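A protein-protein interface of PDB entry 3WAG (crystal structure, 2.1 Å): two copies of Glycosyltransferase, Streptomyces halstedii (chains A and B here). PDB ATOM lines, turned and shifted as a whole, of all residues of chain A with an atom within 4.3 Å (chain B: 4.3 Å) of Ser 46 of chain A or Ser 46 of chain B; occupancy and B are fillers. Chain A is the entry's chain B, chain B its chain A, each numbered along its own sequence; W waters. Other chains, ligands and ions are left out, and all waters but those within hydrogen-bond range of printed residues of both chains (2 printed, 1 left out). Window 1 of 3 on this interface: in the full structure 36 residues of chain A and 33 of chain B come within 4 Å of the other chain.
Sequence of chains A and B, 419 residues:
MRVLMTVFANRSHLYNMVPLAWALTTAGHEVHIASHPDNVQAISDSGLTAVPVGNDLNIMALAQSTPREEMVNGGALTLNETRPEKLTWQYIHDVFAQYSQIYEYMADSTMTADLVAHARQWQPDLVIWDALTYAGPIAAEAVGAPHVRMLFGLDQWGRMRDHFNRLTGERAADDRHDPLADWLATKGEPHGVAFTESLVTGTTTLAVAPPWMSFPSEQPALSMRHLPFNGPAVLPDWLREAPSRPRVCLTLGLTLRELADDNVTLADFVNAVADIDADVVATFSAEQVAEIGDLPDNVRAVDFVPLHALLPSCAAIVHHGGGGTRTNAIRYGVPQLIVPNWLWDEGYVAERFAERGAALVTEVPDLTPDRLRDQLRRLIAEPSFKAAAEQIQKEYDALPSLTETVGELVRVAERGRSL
The backbone NH of Gly 47 of chain B lies within hydrogen-bond range of the backbone carbonyl oxygen of Asp 45 of chain A (3.2 Å).
The indole nitrogen of Trp 22 of chain B lies close to the indole nitrogen of Trp 22 of chain A, 3.3 Å away.
O of Ser 44 of chain A lies close to O of Asp 45 of chain B (2.9 Å).
O of Asp 45 of chain A sits close to O of Ser 44 of chain B (3.2 Å).
Of chain B, only Trp 22, Ser 46 and Gly 47 come within 4 Å of Ser 46 of chain A.
Of chain A, only Ser 46 (3.7 Å) and Gly 47 (3.7 Å) come within 4 Å of Ser 46 of chain B.
Of the printed residues of chain B, Gly 47 of chain A touches Ser 46 (3.7 Å) and Phe 229 (3.2 Å).
Of the printed residues of chain A, Ser 44 of chain B touches Asp 45.
Leu 48 of chain A touches none of the printed residues of chain B.
Ile 43 of chain A touches none of the printed residues of chain B.
Val 18 of chain A touches Trp 22 of chain B, but with the chains exchanged Trp 22 of chain A does not touch Val 18 of chain B (4.03 Å).
Trp 22 of chain A touches Phe 229 of chain B, and with the chains exchanged Phe 229 of chain A touches Trp 22 of chain B.
Ser 46 of chain A touches Gly 47 of chain B, and with the chains exchanged Gly 47 of chain A touches Ser 46 of chain B.
Gly 47 of chain A touches Phe 229 of chain B, and with the chains exchanged Phe 229 of chain A touches Gly 47 of chain B.
Of the 14 pairs that touch across the chains among the printed residues, 11 have their exchanged pair printed and touching as well.
CG1 of Val 18 of chain A touches CH2 of Trp 22 of chain B, 3.8 Å away.
Trp 22 of chain A touches Phe 229 of chain B.
Asp 45 of chain B touches Asp 45 of chain A.
Trp 22 of chain B touches Ser 46 of chain A.
Ser 46 of chain B touches Ser 46 of chain A.
Ser 46 of chain A touches Gly 47 of chain B.
Gly 47 of chain A touches Ser 46 of chain B.
Phe 229 of chain B touches Gly 47 of chain A.
Phe 229 of chain A touches Trp 22 of chain B.
CE1 of Phe 229 of chain A touches O of Gly 47 of chain B, 3.3 Å away.
Printed residues of chain B that touch a printed residue of chain A: Trp 22, Ser 44, Asp 45, Ser 46, Gly 47 and Phe 229.
Hydrophobic or aromatic side chains of chain B within 4 Å of the printed part of chain A: Trp 22 and Phe 229.
Hydrophobic or aromatic side chains of chain A that line the printed part of chain B: Val 18, Trp 22 and Phe 229.
Among the printed residues, no Asp or Glu carboxylate lies within 4 Å of a Lys or Arg side-chain nitrogen of the other chain.
Water W1 bridges the backbone carbonyl oxygen (O) of Trp 22 of chain B (2.7 Å) and the backbone carbonyl oxygen (O) of Trp 22 of chain A (3.1 Å).
Water W2 lies within hydrogen-bond range of O of Ser 44 of chain A (2.9 Å) and O of Asp 45 of chain B (2.9 Å).
The indole nitrogen (NE1) of Trp 22 of chain B sits at hydrogen-bond distance from the backbone carbonyl oxygen (O) of Ser 46 of chain B, at 3.0 Å.
OG of Ser 46 of chain B lies within hydrogen-bond range of O of Ala 42 of chain B, at 2.8 Å.
NE1 of Trp 22 of chain A lies within hydrogen-bond range of O of Ser 46 of chain A (3.0 Å).
The backbone carbonyl oxygen of Ala 42 of chain A sits at hydrogen-bond distance from the side-chain hydroxyl of Ser 46 of chain A (2.9 Å).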
ATOM      1  N   TYR A  15      -5.346  24.616 -27.887  1.00  0.00           N
ATOM      2  CA  TYR A  15      -4.116  23.822 -28.001  1.00  0.00           C
ATOM      3  C   TYR A  15      -3.037  24.533 -27.220  1.00  0.00           C
ATOM      4  O   TYR A  15      -2.145  23.886 -26.641  1.00  0.00           O
ATOM      5  CB  TYR A  15      -3.659  23.767 -29.472  1.00  0.00           C
ATOM      6  CG  TYR A  15      -4.452  22.785 -30.287  1.00  0.00           C
ATOM      7  CD1 TYR A  15      -5.554  22.096 -29.755  1.00  0.00           C
ATOM      8  CD2 TYR A  15      -4.075  22.529 -31.568  1.00  0.00           C
ATOM      9  CE1 TYR A  15      -6.255  21.214 -30.522  1.00  0.00           C
ATOM     10  CE2 TYR A  15      -4.777  21.683 -32.351  1.00  0.00           C
ATOM     11  CZ  TYR A  15      -5.835  21.008 -31.829  1.00  0.00           C
ATOM     12  OH  TYR A  15      -6.438  20.176 -32.695  1.00  0.00           O
ATOM     13  N   VAL A  18      -3.317  23.104 -23.877  1.00  0.00           N
ATOM     14  CA  VAL A  18      -3.459  21.635 -23.715  1.00  0.00           C
ATOM     15  C   VAL A  18      -2.314  21.019 -22.887  1.00  0.00           C
ATOM     16  O   VAL A  18      -2.595  20.281 -21.994  1.00  0.00           O
ATOM     17  CB  VAL A  18      -3.649  20.836 -25.048  1.00  0.00           C
ATOM     18  CG1 VAL A  18      -3.351  19.324 -24.862  1.00  0.00           C
ATOM     19  CG2 VAL A  18      -5.076  21.046 -25.569  1.00  0.00           C
ATOM     20  N   TRP A  22      -2.527  19.054 -19.217  1.00  0.00           N
ATOM     21  CA  TRP A  22      -2.039  17.725 -18.948  1.00  0.00           C
ATOM     22  C   TRP A  22      -0.921  17.610 -17.891  1.00  0.00           C
ATOM     23  O   TRP A  22      -0.901  16.637 -17.145  1.00  0.00           O
ATOM     24  CB  TRP A  22      -1.594  17.078 -20.253  1.00  0.00           C
ATOM     25  CG  TRP A  22      -2.665  16.155 -20.830  1.00  0.00           C
ATOM     26  CD1 TRP A  22      -3.406  16.334 -22.000  1.00  0.00           C
ATOM     27  CD2 TRP A  22      -3.175  14.894 -20.246  1.00  0.00           C
ATOM     28  NE1 TRP A  22      -4.291  15.292 -22.184  1.00  0.00           N
ATOM     29  CE2 TRP A  22      -4.184  14.384 -21.179  1.00  0.00           C
ATOM     30  CE3 TRP A  22      -2.865  14.136 -19.101  1.00  0.00           C
ATOM     31  CZ2 TRP A  22      -4.871  13.175 -20.951  1.00  0.00           C
ATOM     32  CZ3 TRP A  22      -3.544  12.909 -18.882  1.00  0.00           C
ATOM     33  CH2 TRP A  22      -4.522  12.444 -19.805  1.00  0.00           C
ATOM     34  N   ALA A  42     -13.148  19.218 -29.602  1.00  0.00           N
ATOM     35  CA  ALA A  42     -11.718  19.519 -29.607  1.00  0.00           C
ATOM     36  C   ALA A  42     -11.093  19.198 -28.224  1.00  0.00           C
ATOM     37  O   ALA A  42      -9.952  18.688 -28.148  1.00  0.00           O
ATOM     38  CB  ALA A  42     -11.481  20.975 -29.977  1.00  0.00           C
ATOM     39  N   ILE A  43     -11.850  19.452 -27.153  1.00  0.00           N
ATOM     40  CA  ILE A  43     -11.313  19.264 -25.817  1.00  0.00           C
ATOM     41  C   ILE A  43     -11.164  17.765 -25.584  1.00  0.00           C
ATOM     42  O   ILE A  43     -10.093  17.337 -25.173  1.00  0.00           O
ATOM     43  CB  ILE A  43     -12.154  19.956 -24.702  1.00  0.00           C
ATOM     44  CG1 ILE A  43     -12.125  21.500 -24.827  1.00  0.00           C
ATOM     45  CG2 ILE A  43     -11.639  19.503 -23.339  1.00  0.00           C
ATOM     46  CD1 ILE A  43     -13.221  22.223 -24.083  1.00  0.00           C
ATOM     47  N   SER A  44     -12.223  16.971 -25.849  1.00  0.00           N
ATOM     48  CA  SER A  44     -12.086  15.517 -25.807  1.00  0.00           C
ATOM     49  C   SER A  44     -10.985  14.965 -26.651  1.00  0.00           C
ATOM     50  O   SER A  44     -10.298  14.019 -26.215  1.00  0.00           O
ATOM     51  CB  SER A  44     -13.328  14.811 -26.341  1.00  0.00           C
ATOM     52  OG  SER A  44     -14.344  14.976 -25.463  1.00  0.00           O
ATOM     53  N   ASP A  45     -10.865  15.445 -27.897  1.00  0.00           N
ATOM     54  CA  ASP A  45      -9.762  14.905 -28.788  1.00  0.00           C
ATOM     55  C   ASP A  45      -8.351  15.217 -28.295  1.00  0.00           C
ATOM     56  O   ASP A  45      -7.352  14.709 -28.886  1.00  0.00           O
ATOM     57  CB  ASP A  45      -9.867  15.357 -30.227  1.00  0.00           C
ATOM     58  CG  ASP A  45     -11.174  14.882 -30.917  1.00  0.00           C
ATOM     59  OD1 ASP A  45     -11.823  13.912 -30.409  1.00  0.00           O
ATOM     60  OD2 ASP A  45     -11.537  15.562 -31.915  1.00  0.00           O
ATOM     61  N   SER A  46      -8.286  16.077 -27.265  1.00  0.00           N
ATOM     62  CA  SER A  46      -7.039  16.399 -26.613  1.00  0.00           C
ATOM     63  C   SER A  46      -6.820  15.542 -25.355  1.00  0.00           C
ATOM     64  O   SER A  46      -5.812  15.680 -24.688  1.00  0.00           O
ATOM     65  CB  SER A  46      -7.058  17.839 -26.194  1.00  0.00           C
ATOM     66  OG  SER A  46      -7.180  18.594 -27.342  1.00  0.00           O
ATOM     67  N   GLY A  47      -7.806  14.715 -25.016  1.00  0.00           N
ATOM     68  CA  GLY A  47      -7.761  13.845 -23.866  1.00  0.00           C
ATOM     69  C   GLY A  47      -8.110  14.540 -22.566  1.00  0.00           C
ATOM     70  O   GLY A  47      -7.820  14.009 -21.504  1.00  0.00           O
ATOM     71  N   LEU A  48      -8.807  15.669 -22.643  1.00  0.00           N
ATOM     72  CA  LEU A  48      -9.127  16.502 -21.488  1.00  0.00           C
ATOM     73  C   LEU A  48     -10.647  16.486 -21.198  1.00  0.00           C
ATOM     74  O   LEU A  48     -11.471  15.911 -21.997  1.00  0.00           O
ATOM     75  CB  LEU A  48      -8.571  17.947 -21.670  1.00  0.00           C
ATOM     76  CG  LEU A  48      -7.043  17.977 -21.823  1.00  0.00           C
ATOM     77  CD1 LEU A  48      -6.483  19.358 -22.196  1.00  0.00           C
ATOM     78  CD2 LEU A  48      -6.421  17.599 -20.474  1.00  0.00           C
ATOM     79  N   PHE A 229       1.302  22.190 -28.757  1.00  0.00           N
ATOM     80  CA  PHE A 229       0.563  20.924 -29.015  1.00  0.00           C
ATOM     81  C   PHE A 229       0.020  21.072 -30.489  1.00  0.00           C
ATOM     82  O   PHE A 229      -0.593  22.096 -30.815  1.00  0.00           O
ATOM     83  CB  PHE A 229      -0.564  20.778 -27.982  1.00  0.00           C
ATOM     84  CG  PHE A 229      -1.536  19.624 -28.254  1.00  0.00           C
ATOM     85  CD1 PHE A 229      -1.137  18.296 -28.145  1.00  0.00           C
ATOM     86  CD2 PHE A 229      -2.886  19.914 -28.578  1.00  0.00           C
ATOM     87  CE1 PHE A 229      -2.038  17.268 -28.377  1.00  0.00           C
ATOM     88  CE2 PHE A 229      -3.799  18.899 -28.788  1.00  0.00           C
ATOM     89  CZ  PHE A 229      -3.381  17.569 -28.698  1.00  0.00           C
ATOM     90  N   VAL B  18      -2.446   5.848 -21.029  1.00  0.00           N
ATOM     91  CA  VAL B  18      -2.566   7.231 -21.573  1.00  0.00           C
ATOM     92  C   VAL B  18      -1.957   8.314 -20.624  1.00  0.00           C
ATOM     93  O   VAL B  18      -1.265   9.199 -21.047  1.00  0.00           O
ATOM     94  CB  VAL B  18      -4.062   7.598 -21.885  1.00  0.00           C
ATOM     95  CG1 VAL B  18      -4.259   9.072 -22.004  1.00  0.00           C
ATOM     96  CG2 VAL B  18      -4.531   6.945 -23.190  1.00  0.00           C
ATOM     97  N   TRP B  22       1.173  10.894 -21.462  1.00  0.00           N
ATOM     98  CA  TRP B  22       1.140  12.292 -21.248  1.00  0.00           C
ATOM     99  C   TRP B  22       2.198  12.853 -20.292  1.00  0.00           C
ATOM    100  O   TRP B  22       2.672  13.963 -20.507  1.00  0.00           O
ATOM    101  CB  TRP B  22      -0.274  12.726 -20.888  1.00  0.00           C
ATOM    102  CG  TRP B  22      -1.046  13.092 -22.137  1.00  0.00           C
ATOM    103  CD1 TRP B  22      -2.091  12.377 -22.780  1.00  0.00           C
ATOM    104  CD2 TRP B  22      -0.829  14.280 -22.963  1.00  0.00           C
ATOM    105  NE1 TRP B  22      -2.508  13.059 -23.897  1.00  0.00           N
ATOM    106  CE2 TRP B  22      -1.785  14.185 -24.083  1.00  0.00           C
ATOM    107  CE3 TRP B  22       0.053  15.389 -22.897  1.00  0.00           C
ATOM    108  CZ2 TRP B  22      -1.883  15.191 -25.056  1.00  0.00           C
ATOM    109  CZ3 TRP B  22      -0.048  16.395 -23.894  1.00  0.00           C
ATOM    110  CH2 TRP B  22      -0.995  16.289 -24.960  1.00  0.00           C
ATOM    111  N   ALA B  42      -8.488   5.812 -31.490  1.00  0.00           N
ATOM    112  CA  ALA B  42      -8.615   6.005 -30.026  1.00  0.00           C
ATOM    113  C   ALA B  42      -7.332   6.716 -29.446  1.00  0.00           C
ATOM    114  O   ALA B  42      -7.439   7.613 -28.583  1.00  0.00           O
ATOM    115  CB  ALA B  42      -8.977   4.699 -29.321  1.00  0.00           C
ATOM    116  N   ILE B  43      -6.168   6.384 -30.003  1.00  0.00           N
ATOM    117  CA  ILE B  43      -4.899   7.017 -29.619  1.00  0.00           C
ATOM    118  C   ILE B  43      -4.883   8.485 -29.966  1.00  0.00           C
ATOM    119  O   ILE B  43      -4.634   9.349 -29.105  1.00  0.00           O
ATOM    120  CB  ILE B  43      -3.708   6.351 -30.304  1.00  0.00           C
ATOM    121  CG1 ILE B  43      -3.495   4.964 -29.709  1.00  0.00           C
ATOM    122  CG2 ILE B  43      -2.462   7.284 -30.227  1.00  0.00           C
ATOM    123  CD1 ILE B  43      -2.698   4.094 -30.671  1.00  0.00           C
ATOM    124  N   SER B  44      -5.198   8.778 -31.221  1.00  0.00           N
ATOM    125  CA  SER B  44      -5.414  10.175 -31.625  1.00  0.00           C
ATOM    126  C   SER B  44      -6.425  10.953 -30.771  1.00  0.00           C
ATOM    127  O   SER B  44      -6.149  12.077 -30.333  1.00  0.00           O
ATOM    128  CB  SER B  44      -5.864  10.209 -33.104  1.00  0.00           C
ATOM    129  OG  SER B  44      -5.961  11.549 -33.508  1.00  0.00           O
ATOM    130  N   ASP B  45      -7.574  10.331 -30.511  1.00  0.00           N
ATOM    131  CA  ASP B  45      -8.628  10.906 -29.665  1.00  0.00           C
ATOM    132  C   ASP B  45      -8.314  11.069 -28.174  1.00  0.00           C
ATOM    133  O   ASP B  45      -9.077  11.715 -27.432  1.00  0.00           O
ATOM    134  CB  ASP B  45      -9.863  10.012 -29.750  1.00  0.00           C
ATOM    135  CG  ASP B  45     -10.553  10.039 -31.144  1.00  0.00           C
ATOM    136  OD1 ASP B  45     -10.267  10.894 -32.035  1.00  0.00           O
ATOM    137  OD2 ASP B  45     -11.438   9.180 -31.316  1.00  0.00           O
ATOM    138  N   SER B  46      -7.185  10.510 -27.732  1.00  0.00           N
ATOM    139  CA  SER B  46      -6.651  10.776 -26.368  1.00  0.00           C
ATOM    140  C   SER B  46      -5.594  11.898 -26.405  1.00  0.00           C
ATOM    141  O   SER B  46      -4.907  12.152 -25.423  1.00  0.00           O
ATOM    142  CB  SER B  46      -5.972   9.527 -25.891  1.00  0.00           C
ATOM    143  OG  SER B  46      -6.865   8.420 -25.988  1.00  0.00           O
ATOM    144  N   GLY B  47      -5.465  12.568 -27.545  1.00  0.00           N
ATOM    145  CA  GLY B  47      -4.445  13.601 -27.697  1.00  0.00           C
ATOM    146  C   GLY B  47      -3.029  13.157 -28.097  1.00  0.00           C
ATOM    147  O   GLY B  47      -2.108  13.986 -28.116  1.00  0.00           O
ATOM    148  N   LEU B  48      -2.826  11.884 -28.413  1.00  0.00           N
ATOM    149  CA  LEU B  48      -1.465  11.380 -28.592  1.00  0.00           C
ATOM    150  C   LEU B  48      -1.181  11.105 -30.045  1.00  0.00           C
ATOM    151  O   LEU B  48      -2.096  11.198 -30.899  1.00  0.00           O
ATOM    152  CB  LEU B  48      -1.238  10.085 -27.722  1.00  0.00           C
ATOM    153  CG  LEU B  48      -1.444  10.280 -26.195  1.00  0.00           C
ATOM    154  CD1 LEU B  48      -1.768   8.982 -25.424  1.00  0.00           C
ATOM    155  CD2 LEU B  48      -0.282  11.046 -25.573  1.00  0.00           C
ATOM    156  N   PHE B 229      -7.535   6.676 -16.713  1.00  0.00           N
ATOM    157  CA  PHE B 229      -8.034   7.636 -17.738  1.00  0.00           C
ATOM    158  C   PHE B 229      -9.312   7.063 -18.275  1.00  0.00           C
ATOM    159  O   PHE B 229      -9.365   5.887 -18.626  1.00  0.00           O
ATOM    160  CB  PHE B 229      -7.041   7.761 -18.873  1.00  0.00           C
ATOM    161  CG  PHE B 229      -7.515   8.635 -20.043  1.00  0.00           C
ATOM    162  CD1 PHE B 229      -7.611  10.036 -19.923  1.00  0.00           C
ATOM    163  CD2 PHE B 229      -7.868   8.026 -21.274  1.00  0.00           C
ATOM    164  CE1 PHE B 229      -7.984  10.800 -21.046  1.00  0.00           C
ATOM    165  CE2 PHE B 229      -8.256   8.778 -22.383  1.00  0.00           C
ATOM    166  CZ  PHE B 229      -8.290  10.167 -22.271  1.00  0.00           C
HETATM  167  O   HOH W   1       1.463  15.109 -18.428  1.00  0.00           O
HETATM  168  O   HOH W   2     -10.289  11.506 -24.800  1.00  0.00           O
